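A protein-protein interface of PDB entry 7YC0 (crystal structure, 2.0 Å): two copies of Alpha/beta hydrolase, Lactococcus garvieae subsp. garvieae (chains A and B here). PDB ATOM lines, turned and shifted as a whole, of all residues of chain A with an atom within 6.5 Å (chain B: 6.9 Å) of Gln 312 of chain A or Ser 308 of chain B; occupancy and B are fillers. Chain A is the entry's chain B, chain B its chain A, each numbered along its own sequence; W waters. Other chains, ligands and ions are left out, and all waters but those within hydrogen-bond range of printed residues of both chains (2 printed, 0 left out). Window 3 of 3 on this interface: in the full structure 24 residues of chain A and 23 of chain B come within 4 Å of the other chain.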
ATOM      1  N   ARG A 110       7.177 -13.901  22.108  1.00  0.00           N
ATOM      2  CA  ARG A 110       8.020 -13.130  21.153  1.00  0.00           C
ATOM      3  C   ARG A 110       7.979 -13.776  19.770  1.00  0.00           C
ATOM      4  O   ARG A 110       8.245 -13.062  18.801  1.00  0.00           O
ATOM      5  CB  ARG A 110       9.452 -12.991  21.679  1.00  0.00           C
ATOM      6  CG  ARG A 110       9.520 -12.293  23.028  1.00  0.00           C
ATOM      7  CD  ARG A 110      10.917 -11.908  23.458  1.00  0.00           C
ATOM      8  NE  ARG A 110      11.584 -11.003  22.535  1.00  0.00           N
ATOM      9  CZ  ARG A 110      12.813 -10.541  22.719  1.00  0.00           C
ATOM     10  NH1 ARG A 110      13.356  -9.712  21.844  1.00  0.00           N
ATOM     11  NH2 ARG A 110      13.497 -10.907  23.785  1.00  0.00           N
ATOM     12  N   THR A 111       7.684 -15.072  19.648  1.00  0.00           N
ATOM     13  CA  THR A 111       7.550 -15.738  18.318  1.00  0.00           C
ATOM     14  C   THR A 111       6.070 -15.776  17.908  1.00  0.00           C
ATOM     15  O   THR A 111       5.783 -16.097  16.717  1.00  0.00           O
ATOM     16  CB  THR A 111       8.200 -17.129  18.365  1.00  0.00           C
ATOM     17  OG1 THR A 111       7.536 -17.884  19.379  1.00  0.00           O
ATOM     18  CG2 THR A 111       9.678 -17.053  18.699  1.00  0.00           C
ATOM     19  N   MET A 307      17.970 -14.289  23.388  1.00  0.00           N
ATOM     20  CA  MET A 307      16.487 -14.296  23.209  1.00  0.00           C
ATOM     21  C   MET A 307      16.112 -13.439  21.993  1.00  0.00           C
ATOM     22  O   MET A 307      15.332 -13.914  21.130  1.00  0.00           O
ATOM     23  CB  MET A 307      15.780 -13.807  24.479  1.00  0.00           C
ATOM     24  CG  MET A 307      15.971 -14.739  25.668  1.00  0.00           C
ATOM     25  SD  MET A 307      15.719 -16.537  25.342  1.00  0.00           S
ATOM     26  CE  MET A 307      14.205 -16.520  24.382  1.00  0.00           C
ATOM     27  N   SER A 308      16.719 -12.263  21.837  1.00  0.00           N
ATOM     28  CA  SER A 308      16.431 -11.348  20.700  1.00  0.00           C
ATOM     29  C   SER A 308      16.811 -12.037  19.390  1.00  0.00           C
ATOM     30  O   SER A 308      15.976 -12.110  18.509  1.00  0.00           O
ATOM     31  CB  SER A 308      17.089  -9.986  20.860  1.00  0.00           C
ATOM     32  OG  SER A 308      17.310  -9.417  19.578  1.00  0.00           O
ATOM     33  N   LEU A 309      18.001 -12.627  19.299  1.00  0.00           N
ATOM     34  CA  LEU A 309      18.470 -13.296  18.050  1.00  0.00           C
ATOM     35  C   LEU A 309      17.603 -14.536  17.741  1.00  0.00           C
ATOM     36  O   LEU A 309      17.153 -14.696  16.572  1.00  0.00           O
ATOM     37  CB  LEU A 309      19.957 -13.663  18.194  1.00  0.00           C
ATOM     38  CG  LEU A 309      20.536 -14.481  17.045  1.00  0.00           C
ATOM     39  CD1 LEU A 309      20.742 -13.609  15.823  1.00  0.00           C
ATOM     40  CD2 LEU A 309      21.843 -15.148  17.443  1.00  0.00           C
ATOM     41  N   SER A 310      17.402 -15.418  18.713  1.00  0.00           N
ATOM     42  CA  SER A 310      16.713 -16.719  18.479  1.00  0.00           C
ATOM     43  C   SER A 310      15.221 -16.464  18.166  1.00  0.00           C
ATOM     44  O   SER A 310      14.716 -17.068  17.229  1.00  0.00           O
ATOM     45  CB  SER A 310      16.947 -17.689  19.609  1.00  0.00           C
ATOM     46  OG  SER A 310      16.387 -17.257  20.841  1.00  0.00           O
ATOM     47  N   THR A 311      14.553 -15.531  18.847  1.00  0.00           N
ATOM     48  CA  THR A 311      13.125 -15.219  18.566  1.00  0.00           C
ATOM     49  C   THR A 311      12.994 -14.634  17.157  1.00  0.00           C
ATOM     50  O   THR A 311      12.113 -15.143  16.426  1.00  0.00           O
ATOM     51  CB  THR A 311      12.486 -14.365  19.654  1.00  0.00           C
ATOM     52  OG1 THR A 311      13.195 -13.138  19.853  1.00  0.00           O
ATOM     53  CG2 THR A 311      12.406 -15.144  20.944  1.00  0.00           C
ATOM     54  N   GLN A 312      13.855 -13.683  16.753  1.00  0.00           N
ATOM     55  CA  GLN A 312      13.809 -13.053  15.394  1.00  0.00           C
ATOM     56  C   GLN A 312      14.132 -14.091  14.318  1.00  0.00           C
ATOM     57  O   GLN A 312      13.521 -14.047  13.217  1.00  0.00           O
ATOM     58  CB  GLN A 312      14.804 -11.893  15.217  1.00  0.00           C
ATOM     59  CG  GLN A 312      14.621 -10.733  16.189  1.00  0.00           C
ATOM     60  CD  GLN A 312      15.597  -9.606  15.897  1.00  0.00           C
ATOM     61  OE1 GLN A 312      16.529  -9.326  16.664  1.00  0.00           O
ATOM     62  NE2 GLN A 312      15.404  -8.957  14.755  1.00  0.00           N
ATOM     63  N   TRP A 313      15.118 -14.952  14.580  1.00  0.00           N
ATOM     64  CA  TRP A 313      15.503 -16.070  13.672  1.00  0.00           C
ATOM     65  C   TRP A 313      14.298 -17.000  13.390  1.00  0.00           C
ATOM     66  O   TRP A 313      14.095 -17.366  12.191  1.00  0.00           O
ATOM     67  CB  TRP A 313      16.698 -16.845  14.268  1.00  0.00           C
ATOM     68  CG  TRP A 313      17.333 -17.809  13.325  1.00  0.00           C
ATOM     69  CD1 TRP A 313      18.307 -17.529  12.413  1.00  0.00           C
ATOM     70  CD2 TRP A 313      17.067 -19.223  13.215  1.00  0.00           C
ATOM     71  NE1 TRP A 313      18.664 -18.667  11.741  1.00  0.00           N
ATOM     72  CE2 TRP A 313      17.917 -19.721  12.208  1.00  0.00           C
ATOM     73  CE3 TRP A 313      16.216 -20.119  13.875  1.00  0.00           C
ATOM     74  CZ2 TRP A 313      17.946 -21.068  11.858  1.00  0.00           C
ATOM     75  CZ3 TRP A 313      16.231 -21.451  13.511  1.00  0.00           C
ATOM     76  CH2 TRP A 313      17.096 -21.917  12.525  1.00  0.00           C
ATOM     77  N   ILE A 314      13.524 -17.352  14.425  1.00  0.00           N
ATOM     78  CA  ILE A 314      12.305 -18.225  14.329  1.00  0.00           C
ATOM     79  C   ILE A 314      11.206 -17.463  13.571  1.00  0.00           C
ATOM     80  O   ILE A 314      10.644 -18.055  12.629  1.00  0.00           O
ATOM     81  CB  ILE A 314      11.767 -18.703  15.695  1.00  0.00           C
ATOM     82  CG1 ILE A 314      12.710 -19.668  16.420  1.00  0.00           C
ATOM     83  CG2 ILE A 314      10.395 -19.336  15.513  1.00  0.00           C
ATOM     84  CD1 ILE A 314      12.605 -19.597  17.934  1.00  0.00           C
ATOM     85  N   ASN A 315      10.921 -16.210  13.954  1.00  0.00           N
ATOM     86  CA  ASN A 315       9.936 -15.357  13.234  1.00  0.00           C
ATOM     87  C   ASN A 315      10.297 -15.312  11.747  1.00  0.00           C
ATOM     88  O   ASN A 315       9.397 -15.566  10.920  1.00  0.00           O
ATOM     89  CB  ASN A 315       9.828 -13.952  13.814  1.00  0.00           C
ATOM     90  CG  ASN A 315       9.267 -13.976  15.215  1.00  0.00           C
ATOM     91  OD1 ASN A 315       8.650 -14.947  15.641  1.00  0.00           O
ATOM     92  ND2 ASN A 315       9.504 -12.923  15.964  1.00  0.00           N
ATOM     93  N   GLU A 316      11.553 -15.060  11.388  1.00  0.00           N
ATOM     94  CA  GLU A 316      11.888 -14.937   9.949  1.00  0.00           C
ATOM     95  C   GLU A 316      11.602 -16.278   9.257  1.00  0.00           C
ATOM     96  O   GLU A 316      11.261 -16.262   8.042  1.00  0.00           O
ATOM     97  CB  GLU A 316      13.326 -14.471   9.743  1.00  0.00           C
ATOM     98  CG  GLU A 316      13.621 -14.119   8.296  1.00  0.00           C
ATOM     99  CD  GLU A 316      14.058 -15.257   7.390  1.00  0.00           C
ATOM    100  OE1 GLU A 316      14.285 -16.398   7.892  1.00  0.00           O
ATOM    101  OE2 GLU A 316      14.192 -15.005   6.166  1.00  0.00           O
ATOM    102  N   LYS A 317      11.740 -17.400   9.980  1.00  0.00           N
ATOM    103  CA  LYS A 317      11.508 -18.758   9.401  1.00  0.00           C
ATOM    104  C   LYS A 317      10.019 -18.943   9.085  1.00  0.00           C
ATOM    105  O   LYS A 317       9.702 -19.488   8.010  1.00  0.00           O
ATOM    106  CB  LYS A 317      11.993 -19.872  10.333  1.00  0.00           C
ATOM    107  CG  LYS A 317      13.499 -20.096  10.362  1.00  0.00           C
ATOM    108  CD  LYS A 317      14.091 -20.331   9.005  1.00  0.00           C
ATOM    109  CE  LYS A 317      15.595 -20.449   9.050  1.00  0.00           C
ATOM    110  NZ  LYS A 317      16.105 -21.041   7.797  1.00  0.00           N
ATOM    111  N   GLU B 106      20.405  -0.319   5.274  1.00  0.00           N
ATOM    112  CA  GLU B 106      19.807  -1.368   6.139  1.00  0.00           C
ATOM    113  C   GLU B 106      19.643  -0.818   7.552  1.00  0.00           C
ATOM    114  O   GLU B 106      18.574  -1.076   8.159  1.00  0.00           O
ATOM    115  CB  GLU B 106      20.615  -2.664   6.129  1.00  0.00           C
ATOM    116  CG  GLU B 106      20.029  -3.668   7.094  1.00  0.00           C
ATOM    117  CD  GLU B 106      20.319  -5.130   6.841  1.00  0.00           C
ATOM    118  OE1 GLU B 106      21.120  -5.440   5.959  1.00  0.00           O
ATOM    119  OE2 GLU B 106      19.727  -5.949   7.548  1.00  0.00           O
ATOM    120  N   ARG B 110      15.861  -0.421   9.172  1.00  0.00           N
ATOM    121  CA  ARG B 110      15.475  -1.408  10.232  1.00  0.00           C
ATOM    122  C   ARG B 110      15.540  -0.785  11.619  1.00  0.00           C
ATOM    123  O   ARG B 110      14.921  -1.356  12.522  1.00  0.00           O
ATOM    124  CB  ARG B 110      16.309  -2.684  10.145  1.00  0.00           C
ATOM    125  CG  ARG B 110      16.067  -3.458   8.862  1.00  0.00           C
ATOM    126  CD  ARG B 110      16.833  -4.759   8.857  1.00  0.00           C
ATOM    127  NE  ARG B 110      16.263  -5.726   9.775  1.00  0.00           N
ATOM    128  CZ  ARG B 110      16.806  -6.909  10.057  1.00  0.00           C
ATOM    129  NH1 ARG B 110      16.210  -7.726  10.904  1.00  0.00           N
ATOM    130  NH2 ARG B 110      17.957  -7.270   9.513  1.00  0.00           N
ATOM    131  N   ALA B 302      25.805 -15.333   9.279  1.00  0.00           N
ATOM    132  CA  ALA B 302      26.491 -14.370  10.170  1.00  0.00           C
ATOM    133  C   ALA B 302      25.962 -12.966   9.877  1.00  0.00           C
ATOM    134  O   ALA B 302      25.576 -12.294  10.819  1.00  0.00           O
ATOM    135  CB  ALA B 302      27.989 -14.431   9.973  1.00  0.00           C
ATOM    136  N   THR B 303      25.932 -12.540   8.609  1.00  0.00           N
ATOM    137  CA  THR B 303      25.491 -11.163   8.266  1.00  0.00           C
ATOM    138  C   THR B 303      24.026 -10.995   8.708  1.00  0.00           C
ATOM    139  O   THR B 303      23.715 -10.001   9.394  1.00  0.00           O
ATOM    140  CB  THR B 303      25.728 -10.848   6.784  1.00  0.00           C
ATOM    141  OG1 THR B 303      27.121 -10.989   6.470  1.00  0.00           O
ATOM    142  CG2 THR B 303      25.272  -9.457   6.404  1.00  0.00           C
ATOM    143  N   ARG B 304      23.144 -11.933   8.352  1.00  0.00           N
ATOM    144  CA  ARG B 304      21.691 -11.806   8.667  1.00  0.00           C
ATOM    145  C   ARG B 304      21.548 -11.701  10.192  1.00  0.00           C
ATOM    146  O   ARG B 304      20.860 -10.782  10.681  1.00  0.00           O
ATOM    147  CB  ARG B 304      20.910 -12.969   8.037  1.00  0.00           C
ATOM    148  CG  ARG B 304      20.871 -12.930   6.514  1.00  0.00           C
ATOM    149  CD  ARG B 304      20.229 -11.656   5.987  1.00  0.00           C
ATOM    150  NE  ARG B 304      21.131 -10.571   5.545  1.00  0.00           N
ATOM    151  CZ  ARG B 304      21.038  -9.292   5.921  1.00  0.00           C
ATOM    152  NH1 ARG B 304      21.822  -8.370   5.395  1.00  0.00           N
ATOM    153  NH2 ARG B 304      20.153  -8.929   6.819  1.00  0.00           N
ATOM    154  N   ALA B 305      22.267 -12.523  10.947  1.00  0.00           N
ATOM    155  CA  ALA B 305      22.149 -12.572  12.424  1.00  0.00           C
ATOM    156  C   ALA B 305      22.780 -11.326  13.059  1.00  0.00           C
ATOM    157  O   ALA B 305      22.209 -10.803  14.003  1.00  0.00           O
ATOM    158  CB  ALA B 305      22.786 -13.837  12.951  1.00  0.00           C
ATOM    159  N   ALA B 306      23.935 -10.873  12.564  1.00  0.00           N
ATOM    160  CA  ALA B 306      24.599  -9.636  13.046  1.00  0.00           C
ATOM    161  C   ALA B 306      23.661  -8.440  12.874  1.00  0.00           C
ATOM    162  O   ALA B 306      23.565  -7.627  13.799  1.00  0.00           O
ATOM    163  CB  ALA B 306      25.893  -9.401  12.312  1.00  0.00           C
ATOM    164  N   MET B 307      23.011  -8.318  11.714  1.00  0.00           N
ATOM    165  CA  MET B 307      22.131  -7.155  11.440  1.00  0.00           C
ATOM    166  C   MET B 307      20.864  -7.256  12.305  1.00  0.00           C
ATOM    167  O   MET B 307      20.463  -6.212  12.845  1.00  0.00           O
ATOM    168  CB  MET B 307      21.786  -7.065   9.957  1.00  0.00           C
ATOM    169  CG  MET B 307      22.990  -6.820   9.063  1.00  0.00           C
ATOM    170  SD  MET B 307      23.991  -5.406   9.566  1.00  0.00           S
ATOM    171  CE  MET B 307      22.768  -4.098   9.553  1.00  0.00           C
ATOM    172  N   SER B 308      20.287  -8.457  12.486  1.00  0.00           N
ATOM    173  CA  SER B 308      19.106  -8.664  13.370  1.00  0.00           C
ATOM    174  C   SER B 308      19.472  -8.278  14.793  1.00  0.00           C
ATOM    175  O   SER B 308      18.687  -7.555  15.439  1.00  0.00           O
ATOM    176  CB  SER B 308      18.558 -10.081  13.329  1.00  0.00           C
ATOM    177  OG  SER B 308      18.147 -10.387  12.006  1.00  0.00           O
ATOM    178  N   LEU B 309      20.616  -8.759  15.278  1.00  0.00           N
ATOM    179  CA  LEU B 309      21.059  -8.442  16.653  1.00  0.00           C
ATOM    180  C   LEU B 309      21.277  -6.932  16.761  1.00  0.00           C
ATOM    181  O   LEU B 309      20.701  -6.303  17.691  1.00  0.00           O
ATOM    182  CB  LEU B 309      22.327  -9.217  17.020  1.00  0.00           C
ATOM    183  CG  LEU B 309      22.818  -8.939  18.441  1.00  0.00           C
ATOM    184  CD1 LEU B 309      21.792  -9.399  19.453  1.00  0.00           C
ATOM    185  CD2 LEU B 309      24.162  -9.597  18.708  1.00  0.00           C
ATOM    186  N   SER B 310      22.044  -6.340  15.848  1.00  0.00           N
ATOM    187  CA  SER B 310      22.455  -4.912  15.998  1.00  0.00           C
ATOM    188  C   SER B 310      21.237  -3.966  15.890  1.00  0.00           C
ATOM    189  O   SER B 310      21.137  -3.046  16.731  1.00  0.00           O
ATOM    190  CB  SER B 310      23.599  -4.517  15.090  1.00  0.00           C
ATOM    191  OG  SER B 310      23.394  -4.865  13.738  1.00  0.00           O
ATOM    192  N   THR B 311      20.348  -4.181  14.921  1.00  0.00           N
ATOM    193  CA  THR B 311      19.172  -3.291  14.680  1.00  0.00           C
ATOM    194  C   THR B 311      18.225  -3.400  15.882  1.00  0.00           C
ATOM    195  O   THR B 311      17.868  -2.353  16.470  1.00  0.00           O
ATOM    196  CB  THR B 311      18.583  -3.555  13.298  1.00  0.00           C
ATOM    197  OG1 THR B 311      18.137  -4.896  13.146  1.00  0.00           O
ATOM    198  CG2 THR B 311      19.580  -3.235  12.211  1.00  0.00           C
ATOM    199  N   GLN B 312      17.953  -4.616  16.342  1.00  0.00           N
ATOM    200  CA  GLN B 312      17.089  -4.850  17.525  1.00  0.00           C
ATOM    201  C   GLN B 312      17.677  -4.154  18.746  1.00  0.00           C
ATOM    202  O   GLN B 312      16.908  -3.541  19.520  1.00  0.00           O
ATOM    203  CB  GLN B 312      16.965  -6.340  17.825  1.00  0.00           C
ATOM    204  CG  GLN B 312      15.980  -6.632  18.944  1.00  0.00           C
ATOM    205  CD  GLN B 312      14.663  -7.173  18.433  1.00  0.00           C
ATOM    206  OE1 GLN B 312      14.414  -7.236  17.229  1.00  0.00           O
ATOM    207  NE2 GLN B 312      13.808  -7.574  19.361  1.00  0.00           N
ATOM    208  N   TRP B 313      18.980  -4.310  18.972  1.00  0.00           N
ATOM    209  CA  TRP B 313      19.659  -3.777  20.185  1.00  0.00           C
ATOM    210  C   TRP B 313      19.544  -2.250  20.216  1.00  0.00           C
ATOM    211  O   TRP B 313      19.346  -1.664  21.313  1.00  0.00           O
ATOM    212  CB  TRP B 313      21.122  -4.240  20.205  1.00  0.00           C
ATOM    213  CG  TRP B 313      21.925  -3.880  21.410  1.00  0.00           C
ATOM    214  CD1 TRP B 313      22.074  -4.621  22.546  1.00  0.00           C
ATOM    215  CD2 TRP B 313      22.758  -2.720  21.568  1.00  0.00           C
ATOM    216  NE1 TRP B 313      22.926  -3.999  23.408  1.00  0.00           N
ATOM    217  CE2 TRP B 313      23.375  -2.837  22.830  1.00  0.00           C
ATOM    218  CE3 TRP B 313      23.073  -1.628  20.754  1.00  0.00           C
ATOM    219  CZ2 TRP B 313      24.283  -1.895  23.298  1.00  0.00           C
ATOM    220  CZ3 TRP B 313      23.973  -0.696  21.221  1.00  0.00           C
ATOM    221  CH2 TRP B 313      24.576  -0.836  22.474  1.00  0.00           C
HETATM  222  O   HOH W   1      19.411  -7.521  20.241  1.00  0.00           O
HETATM  223  O   HOH W   2      15.711  -5.852  13.876  1.00  0.00           O
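The side-chain amide oxygen (OE1) of Gln 312 of chain A lies close to the backbone carbonyl oxygen (O) of Ser 308 of chain B (3.0 Å).
The side-chain amide nitrogen (NE2) of Gln 312 of chain B sits close to the guanidinium group (NH1) of Arg 110 of chain A (3.3 Å).
The side-chain amide oxygen of Gln 312 of chain B lies close to the side-chain amide oxygen of Gln 312 of chain A (3.0 Å).
NH1 of Arg 110 of chain B lies within hydrogen-bond range of OG of Ser 308 of chain B, 3.5 Å away.
The backbone carbonyl oxygen of Arg 304 of chain B is in hydrogen-bond range of the side-chain hydroxyl of Ser 308 of chain B (3.0 Å).
The backbone carbonyl oxygen (O) of Arg 110 of chain A sits at hydrogen-bond distance from the side-chain amide nitrogen (ND2) of Asn 315 of chain A (3.1 Å).
The side-chain hydroxyl of Thr 311 of chain A is in hydrogen-bond range of the backbone carbonyl oxygen of Ser 308 of chain A.
OE1 of Gln 312 of chain A is in hydrogen-bond range of OG of Ser 308 of chain A.
Ser 308 of chain A touches Gln 312 of chain B (OG to CG, 3.2 Å).
Leu 309 of chain A touches Ala 305 of chain B.
Ser 308 of chain B touches one residue of chain A.
Printed residues of chain B within 4 Å of Ser 308 of chain A: Gln 312.
Of the printed residues of chain A, Gln 312 of chain B touches Arg 110 (3.3 Å), Ser 308 (3.2 Å) and Gln 312 (3.0 Å).
Of the printed residues of chain A, Ala 305 of chain B touches Leu 309.
Ala 306 of chain B touches none of the printed residues of chain A.
The nearest residue of chain A that does not touch Ser 308 of chain B is Ser 308 of chain A (4.7 Å).
Of the 13 printed residues of chain A, 4 touch a printed residue of chain B.
Printed residues of chain A that touch a printed residue of chain B: Arg 110, Ser 308, Leu 309 and Gln 312.
Hydrophobic or aromatic side chains of chain B within 4 Å of the printed part of chain A: Ala 305.
Arg 110 of chain A touches Gln 312 of chain B, but with the chains exchanged Gln 312 of chain A does not touch Arg 110 of chain B (4.1 Å).
Ser 308 of chain A touches Gln 312 of chain B, and with the chains exchanged Gln 312 of chain A touches Ser 308 of chain B.
Gln 312 of chain A touches its own counterpart, Gln 312 of chain B.
8 positions are printed for both chains.
Water W2 lies within hydrogen-bond range of the side-chain hydroxyl of Thr 311 of chain B (2.7 Å) and the side-chain amide nitrogen of Gln 312 of chain A (3.2 Å).
Water W1 lies within hydrogen-bond range of OG of Ser 308 of chain A (2.9 Å), O of Leu 309 of chain B (3.1 Å) and N of Trp 313 of chain B (3.5 Å).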
